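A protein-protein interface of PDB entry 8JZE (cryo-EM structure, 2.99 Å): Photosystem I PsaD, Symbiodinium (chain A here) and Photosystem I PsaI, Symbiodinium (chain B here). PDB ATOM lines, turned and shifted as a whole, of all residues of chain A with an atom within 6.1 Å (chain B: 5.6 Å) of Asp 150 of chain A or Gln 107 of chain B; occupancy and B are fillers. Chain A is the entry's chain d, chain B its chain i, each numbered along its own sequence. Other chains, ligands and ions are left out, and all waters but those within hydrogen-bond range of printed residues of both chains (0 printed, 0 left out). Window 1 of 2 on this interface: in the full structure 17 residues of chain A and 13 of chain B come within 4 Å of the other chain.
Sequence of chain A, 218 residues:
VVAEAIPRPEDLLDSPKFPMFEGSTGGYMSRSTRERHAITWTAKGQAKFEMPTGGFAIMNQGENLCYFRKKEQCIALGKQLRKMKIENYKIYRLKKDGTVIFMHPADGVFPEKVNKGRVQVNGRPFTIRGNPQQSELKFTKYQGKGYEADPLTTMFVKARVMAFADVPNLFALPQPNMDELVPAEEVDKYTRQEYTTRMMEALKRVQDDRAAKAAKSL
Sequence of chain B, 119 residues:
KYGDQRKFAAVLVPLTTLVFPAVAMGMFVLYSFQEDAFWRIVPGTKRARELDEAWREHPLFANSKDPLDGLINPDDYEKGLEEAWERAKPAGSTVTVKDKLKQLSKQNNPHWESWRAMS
The backbone NH (N) of Leu 152 of chain A lies within hydrogen-bond range of the backbone carbonyl oxygen (O) of Leu 104 of chain B. NH1 of Arg 124 of chain A lies within hydrogen-bond range of OE1 of Gln 107 of chain B (3.4 Å). The backbone carbonyl oxygen of Glu 148 of chain A lies within hydrogen-bond range of the side-chain amide nitrogen of Gln 107 of chain B (2.6 Å). NE2 of Gln 107 of chain B sits close to N of Asp 150 of chain A, 3.2 Å away.
The side-chain amide nitrogen (NE2) of Gln 107 of chain B lies close to the side-chain amide nitrogen (ND2) of Asn 109 of chain B. NH1 of Arg 124 of chain A sits at hydrogen-bond distance from O of Tyr 147 of chain A, 2.8 Å away. O of Ala 149 of chain A lies within hydrogen-bond range of NH2 of Arg 124 of chain A (2.4 Å). The side-chain hydroxyl of Tyr 142 of chain A is in hydrogen-bond range of the side-chain carboxylate of Asp 150 of chain A (2.8 Å). OD1 of Asp 150 of chain A lies close to N of Leu 152 of chain A, 3.3 Å away. N of Thr 153 of chain A lies within hydrogen-bond range of OD1 of Asp 150 of chain A (2.7 Å).
Glu 148 of chain A touches Asn 109 of chain B (O to ND2, 3.5 Å). O of Ala 149 of chain A touches OE1 of Gln 107 of chain B (3.5 Å). Asp 150 of chain A touches Leu 104 of chain B. Ser 105 of chain B touches Asp 150 of chain A (O to CB, 3.4 Å). Pro 151 of chain A touches Leu 104 of chain B. Leu 152 of chain A touches Ser 105 of chain B (CD2 to CB, 3.8 Å). Met 155 of chain A touches Leu 104 of chain B (CE to CD1, 3.5 Å).
Of chain A, only Arg 124, Glu 148, Ala 149 and Asp 150 come within 4 Å of Gln 107 of chain B. Of the printed residues of chain B, Leu 152 of chain A touches Leu 104 and Ser 105. Of the printed residues of chain B, Ala 149 of chain A touches Gln 107. Printed residues of chain B within 4 Å of Glu 148 of chain A: Gln 107 and Asn 109. Of the printed residues of chain B, Arg 124 of chain A touches Gln 107 (3.4 Å). Printed residues of chain B within 4 Å of Met 155 of chain A: Leu 104. The nearest residue of chain A that does not touch Gln 107 of chain B is Pro 151 of chain A (4.3 Å).
Of the 14 printed residues of chain A, 7 touch a printed residue of chain B. Hydrophobic or aromatic side chains of chain A that line the printed part of chain B: Pro 151, Leu 152 and Met 155. Among the printed residues, 11 pairs touch across the chains. Among the printed residues, no Asp or Glu carboxylate lies within 4 Å of a Lys or Arg side-chain nitrogen of the other chain.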
ATOM      1  N   GLY A 123      27.097 -20.163 -28.115  1.00  0.00           N
ATOM      2  CA  GLY A 123      26.789 -19.993 -26.707  1.00  0.00           C
ATOM      3  C   GLY A 123      25.535 -20.764 -26.326  1.00  0.00           C
ATOM      4  O   GLY A 123      24.582 -20.849 -27.099  1.00  0.00           O
ATOM      5  N   ARG A 124      25.553 -21.331 -25.122  1.00  0.00           N
ATOM      6  CA  ARG A 124      24.435 -22.113 -24.609  1.00  0.00           C
ATOM      7  C   ARG A 124      24.012 -21.554 -23.257  1.00  0.00           C
ATOM      8  O   ARG A 124      24.840 -21.489 -22.332  1.00  0.00           O
ATOM      9  CB  ARG A 124      24.813 -23.593 -24.498  1.00  0.00           C
ATOM     10  CG  ARG A 124      25.322 -24.183 -25.809  1.00  0.00           C
ATOM     11  CD  ARG A 124      25.348 -25.702 -25.794  1.00  0.00           C
ATOM     12  NE  ARG A 124      24.027 -26.274 -25.566  1.00  0.00           N
ATOM     13  CZ  ARG A 124      23.095 -26.408 -26.499  1.00  0.00           C
ATOM     14  NH1 ARG A 124      23.297 -25.999 -27.740  1.00  0.00           N
ATOM     15  NH2 ARG A 124      21.931 -26.965 -26.178  1.00  0.00           N
ATOM     16  N   PHE A 126      22.862 -22.125 -20.284  1.00  0.00           N
ATOM     17  CA  PHE A 126      22.671 -22.948 -19.094  1.00  0.00           C
ATOM     18  C   PHE A 126      24.002 -23.594 -18.741  1.00  0.00           C
ATOM     19  O   PHE A 126      24.971 -23.516 -19.500  1.00  0.00           O
ATOM     20  CB  PHE A 126      21.585 -24.012 -19.291  1.00  0.00           C
ATOM     21  CG  PHE A 126      21.561 -24.619 -20.665  1.00  0.00           C
ATOM     22  CD1 PHE A 126      22.556 -25.488 -21.076  1.00  0.00           C
ATOM     23  CD2 PHE A 126      20.525 -24.334 -21.537  1.00  0.00           C
ATOM     24  CE1 PHE A 126      22.528 -26.050 -22.335  1.00  0.00           C
ATOM     25  CE2 PHE A 126      20.488 -24.892 -22.796  1.00  0.00           C
ATOM     26  CZ  PHE A 126      21.491 -25.752 -23.195  1.00  0.00           C
ATOM     27  N   LYS A 141      16.163 -33.711 -35.400  1.00  0.00           N
ATOM     28  CA  LYS A 141      17.266 -32.934 -35.959  1.00  0.00           C
ATOM     29  C   LYS A 141      18.577 -33.170 -35.218  1.00  0.00           C
ATOM     30  O   LYS A 141      19.650 -32.946 -35.788  1.00  0.00           O
ATOM     31  CB  LYS A 141      16.937 -31.440 -35.924  1.00  0.00           C
ATOM     32  CG  LYS A 141      15.635 -31.049 -36.600  1.00  0.00           C
ATOM     33  CD  LYS A 141      15.209 -29.644 -36.192  1.00  0.00           C
ATOM     34  CE  LYS A 141      16.338 -28.645 -36.391  1.00  0.00           C
ATOM     35  NZ  LYS A 141      15.958 -27.266 -35.979  1.00  0.00           N
ATOM     36  N   TYR A 142      18.513 -33.634 -33.970  1.00  0.00           N
ATOM     37  CA  TYR A 142      19.685 -33.764 -33.116  1.00  0.00           C
ATOM     38  C   TYR A 142      19.895 -35.223 -32.722  1.00  0.00           C
ATOM     39  O   TYR A 142      20.061 -35.533 -31.538  1.00  0.00           O
ATOM     40  CB  TYR A 142      19.534 -32.886 -31.871  1.00  0.00           C
ATOM     41  CG  TYR A 142      19.018 -31.493 -32.162  1.00  0.00           C
ATOM     42  CD1 TYR A 142      19.784 -30.586 -32.882  1.00  0.00           C
ATOM     43  CD2 TYR A 142      17.769 -31.083 -31.712  1.00  0.00           C
ATOM     44  CE1 TYR A 142      19.321 -29.315 -33.150  1.00  0.00           C
ATOM     45  CE2 TYR A 142      17.298 -29.811 -31.973  1.00  0.00           C
ATOM     46  CZ  TYR A 142      18.079 -28.933 -32.693  1.00  0.00           C
ATOM     47  OH  TYR A 142      17.617 -27.666 -32.960  1.00  0.00           O
ATOM     48  N   TYR A 147      24.040 -31.927 -27.665  1.00  0.00           N
ATOM     49  CA  TYR A 147      24.657 -30.665 -27.275  1.00  0.00           C
ATOM     50  C   TYR A 147      24.411 -29.546 -28.279  1.00  0.00           C
ATOM     51  O   TYR A 147      24.772 -28.399 -28.000  1.00  0.00           O
ATOM     52  CB  TYR A 147      26.164 -30.852 -27.075  1.00  0.00           C
ATOM     53  CG  TYR A 147      26.885 -31.458 -28.259  1.00  0.00           C
ATOM     54  CD1 TYR A 147      27.364 -30.658 -29.289  1.00  0.00           C
ATOM     55  CD2 TYR A 147      27.098 -32.827 -28.341  1.00  0.00           C
ATOM     56  CE1 TYR A 147      28.024 -31.205 -30.367  1.00  0.00           C
ATOM     57  CE2 TYR A 147      27.759 -33.383 -29.415  1.00  0.00           C
ATOM     58  CZ  TYR A 147      28.220 -32.567 -30.425  1.00  0.00           C
ATOM     59  OH  TYR A 147      28.880 -33.116 -31.499  1.00  0.00           O
ATOM     60  N   GLU A 148      23.817 -29.847 -29.432  1.00  0.00           N
ATOM     61  CA  GLU A 148      23.502 -28.842 -30.436  1.00  0.00           C
ATOM     62  C   GLU A 148      22.065 -28.348 -30.352  1.00  0.00           C
ATOM     63  O   GLU A 148      21.672 -27.494 -31.150  1.00  0.00           O
ATOM     64  CB  GLU A 148      23.765 -29.398 -31.840  1.00  0.00           C
ATOM     65  CG  GLU A 148      25.187 -29.881 -32.075  1.00  0.00           C
ATOM     66  CD  GLU A 148      26.144 -28.758 -32.423  1.00  0.00           C
ATOM     67  OE1 GLU A 148      25.743 -27.579 -32.345  1.00  0.00           O
ATOM     68  OE2 GLU A 148      27.303 -29.056 -32.782  1.00  0.00           O
ATOM     69  N   ALA A 149      21.278 -28.860 -29.409  1.00  0.00           N
ATOM     70  CA  ALA A 149      19.869 -28.500 -29.329  1.00  0.00           C
ATOM     71  C   ALA A 149      19.697 -27.050 -28.897  1.00  0.00           C
ATOM     72  O   ALA A 149      20.390 -26.562 -28.000  1.00  0.00           O
ATOM     73  CB  ALA A 149      19.139 -29.422 -28.352  1.00  0.00           C
ATOM     74  N   ASP A 150      18.763 -26.360 -29.548  1.00  0.00           N
ATOM     75  CA  ASP A 150      18.409 -25.015 -29.131  1.00  0.00           C
ATOM     76  C   ASP A 150      17.759 -25.060 -27.749  1.00  0.00           C
ATOM     77  O   ASP A 150      17.121 -26.053 -27.392  1.00  0.00           O
ATOM     78  CB  ASP A 150      17.460 -24.373 -30.141  1.00  0.00           C
ATOM     79  CG  ASP A 150      16.202 -25.188 -30.363  1.00  0.00           C
ATOM     80  OD1 ASP A 150      15.294 -25.133 -29.507  1.00  0.00           O
ATOM     81  OD2 ASP A 150      16.123 -25.882 -31.397  1.00  0.00           O
ATOM     82  N   PRO A 151      17.912 -23.999 -26.951  1.00  0.00           N
ATOM     83  CA  PRO A 151      17.397 -24.049 -25.572  1.00  0.00           C
ATOM     84  C   PRO A 151      15.903 -24.312 -25.488  1.00  0.00           C
ATOM     85  O   PRO A 151      15.448 -24.917 -24.508  1.00  0.00           O
ATOM     86  CB  PRO A 151      17.766 -22.671 -25.005  1.00  0.00           C
ATOM     87  CG  PRO A 151      18.035 -21.812 -26.192  1.00  0.00           C
ATOM     88  CD  PRO A 151      18.587 -22.724 -27.240  1.00  0.00           C
ATOM     89  N   LEU A 152      15.125 -23.881 -26.484  1.00  0.00           N
ATOM     90  CA  LEU A 152      13.698 -24.185 -26.479  1.00  0.00           C
ATOM     91  C   LEU A 152      13.454 -25.686 -26.562  1.00  0.00           C
ATOM     92  O   LEU A 152      12.590 -26.220 -25.859  1.00  0.00           O
ATOM     93  CB  LEU A 152      12.991 -23.462 -27.626  1.00  0.00           C
ATOM     94  CG  LEU A 152      11.484 -23.717 -27.702  1.00  0.00           C
ATOM     95  CD1 LEU A 152      10.823 -23.359 -26.386  1.00  0.00           C
ATOM     96  CD2 LEU A 152      10.848 -22.947 -28.849  1.00  0.00           C
ATOM     97  N   THR A 153      14.205 -26.386 -27.416  1.00  0.00           N
ATOM     98  CA  THR A 153      14.064 -27.836 -27.496  1.00  0.00           C
ATOM     99  C   THR A 153      14.483 -28.502 -26.192  1.00  0.00           C
ATOM    100  O   THR A 153      13.872 -29.492 -25.769  1.00  0.00           O
ATOM    101  CB  THR A 153      14.881 -28.389 -28.663  1.00  0.00           C
ATOM    102  OG1 THR A 153      16.177 -27.778 -28.675  1.00  0.00           O
ATOM    103  CG2 THR A 153      14.178 -28.120 -29.983  1.00  0.00           C
ATOM    104  N   THR A 154      15.529 -27.981 -25.544  1.00  0.00           N
ATOM    105  CA  THR A 154      15.950 -28.537 -24.263  1.00  0.00           C
ATOM    106  C   THR A 154      14.858 -28.381 -23.214  1.00  0.00           C
ATOM    107  O   THR A 154      14.562 -29.324 -22.471  1.00  0.00           O
ATOM    108  CB  THR A 154      17.236 -27.864 -23.789  1.00  0.00           C
ATOM    109  OG1 THR A 154      16.930 -26.567 -23.264  1.00  0.00           O
ATOM    110  CG2 THR A 154      18.209 -27.710 -24.940  1.00  0.00           C
ATOM    111  N   MET A 155      14.235 -27.203 -23.148  1.00  0.00           N
ATOM    112  CA  MET A 155      13.134 -27.010 -22.209  1.00  0.00           C
ATOM    113  C   MET A 155      11.948 -27.900 -22.555  1.00  0.00           C
ATOM    114  O   MET A 155      11.275 -28.423 -21.661  1.00  0.00           O
ATOM    115  CB  MET A 155      12.701 -25.546 -22.185  1.00  0.00           C
ATOM    116  CG  MET A 155      13.634 -24.615 -21.445  1.00  0.00           C
ATOM    117  SD  MET A 155      12.923 -22.963 -21.382  1.00  0.00           S
ATOM    118  CE  MET A 155      12.300 -22.822 -23.052  1.00  0.00           C
ATOM    119  N   GLN B 103      12.979 -16.237 -29.577  1.00  0.00           N
ATOM    120  CA  GLN B 103      14.398 -16.052 -29.305  1.00  0.00           C
ATOM    121  C   GLN B 103      15.016 -17.238 -28.575  1.00  0.00           C
ATOM    122  O   GLN B 103      16.242 -17.389 -28.597  1.00  0.00           O
ATOM    123  CB  GLN B 103      14.623 -14.766 -28.505  1.00  0.00           C
ATOM    124  CG  GLN B 103      14.257 -14.850 -27.032  1.00  0.00           C
ATOM    125  CD  GLN B 103      15.475 -14.997 -26.140  1.00  0.00           C
ATOM    126  OE1 GLN B 103      16.575 -15.272 -26.616  1.00  0.00           O
ATOM    127  NE2 GLN B 103      15.284 -14.810 -24.839  1.00  0.00           N
ATOM    128  N   LEU B 104      14.203 -18.078 -27.929  1.00  0.00           N
ATOM    129  CA  LEU B 104      14.715 -19.313 -27.350  1.00  0.00           C
ATOM    130  C   LEU B 104      14.857 -20.421 -28.382  1.00  0.00           C
ATOM    131  O   LEU B 104      15.575 -21.393 -28.133  1.00  0.00           O
ATOM    132  CB  LEU B 104      13.809 -19.780 -26.208  1.00  0.00           C
ATOM    133  CG  LEU B 104      14.005 -19.064 -24.871  1.00  0.00           C
ATOM    134  CD1 LEU B 104      12.914 -19.426 -23.881  1.00  0.00           C
ATOM    135  CD2 LEU B 104      15.371 -19.395 -24.297  1.00  0.00           C
ATOM    136  N   SER B 105      14.188 -20.299 -29.528  1.00  0.00           N
ATOM    137  CA  SER B 105      14.389 -21.260 -30.604  1.00  0.00           C
ATOM    138  C   SER B 105      15.595 -20.904 -31.460  1.00  0.00           C
ATOM    139  O   SER B 105      16.277 -21.802 -31.967  1.00  0.00           O
ATOM    140  CB  SER B 105      13.137 -21.347 -31.477  1.00  0.00           C
ATOM    141  OG  SER B 105      12.860 -20.100 -32.089  1.00  0.00           O
ATOM    142  N   LYS B 106      15.879 -19.614 -31.624  1.00  0.00           N
ATOM    143  CA  LYS B 106      16.975 -19.149 -32.470  1.00  0.00           C
ATOM    144  C   LYS B 106      18.258 -19.128 -31.649  1.00  0.00           C
ATOM    145  O   LYS B 106      18.463 -18.243 -30.815  1.00  0.00           O
ATOM    146  CB  LYS B 106      16.665 -17.769 -33.040  1.00  0.00           C
ATOM    147  CG  LYS B 106      15.698 -17.770 -34.211  1.00  0.00           C
ATOM    148  CD  LYS B 106      15.294 -16.351 -34.585  1.00  0.00           C
ATOM    149  CE  LYS B 106      16.511 -15.461 -34.786  1.00  0.00           C
ATOM    150  NZ  LYS B 106      16.126 -14.046 -35.050  1.00  0.00           N
ATOM    151  N   GLN B 107      19.126 -20.107 -31.887  1.00  0.00           N
ATOM    152  CA  GLN B 107      20.469 -20.119 -31.332  1.00  0.00           C
ATOM    153  C   GLN B 107      21.470 -19.774 -32.433  1.00  0.00           C
ATOM    154  O   GLN B 107      21.115 -19.606 -33.603  1.00  0.00           O
ATOM    155  CB  GLN B 107      20.780 -21.474 -30.691  1.00  0.00           C
ATOM    156  CG  GLN B 107      20.679 -22.657 -31.639  1.00  0.00           C
ATOM    157  CD  GLN B 107      21.126 -23.956 -30.997  1.00  0.00           C
ATOM    158  OE1 GLN B 107      21.760 -23.955 -29.943  1.00  0.00           O
ATOM    159  NE2 GLN B 107      20.792 -25.074 -31.630  1.00  0.00           N
ATOM    160  N   ASN B 108      22.743 -19.668 -32.055  1.00  0.00           N
ATOM    161  CA  ASN B 108      23.811 -19.256 -32.969  1.00  0.00           C
ATOM    162  C   ASN B 108      24.869 -20.356 -32.997  1.00  0.00           C
ATOM    163  O   ASN B 108      25.839 -20.309 -32.238  1.00  0.00           O
ATOM    164  CB  ASN B 108      24.399 -17.913 -32.539  1.00  0.00           C
ATOM    165  CG  ASN B 108      25.223 -17.254 -33.629  1.00  0.00           C
ATOM    166  OD1 ASN B 108      25.725 -17.917 -34.534  1.00  0.00           O
ATOM    167  ND2 ASN B 108      25.369 -15.937 -33.544  1.00  0.00           N
ATOM    168  N   ASN B 109      24.682 -21.343 -33.873  1.00  0.00           N
ATOM    169  CA  ASN B 109      25.646 -22.425 -34.076  1.00  0.00           C
ATOM    170  C   ASN B 109      25.911 -22.590 -35.568  1.00  0.00           C
ATOM    171  O   ASN B 109      25.436 -23.541 -36.201  1.00  0.00           O
ATOM    172  CB  ASN B 109      25.157 -23.734 -33.453  1.00  0.00           C
ATOM    173  CG  ASN B 109      23.745 -24.098 -33.874  1.00  0.00           C
ATOM    174  OD1 ASN B 109      23.122 -23.405 -34.679  1.00  0.00           O
ATOM    175  ND2 ASN B 109      23.238 -25.199 -33.337  1.00  0.00           N
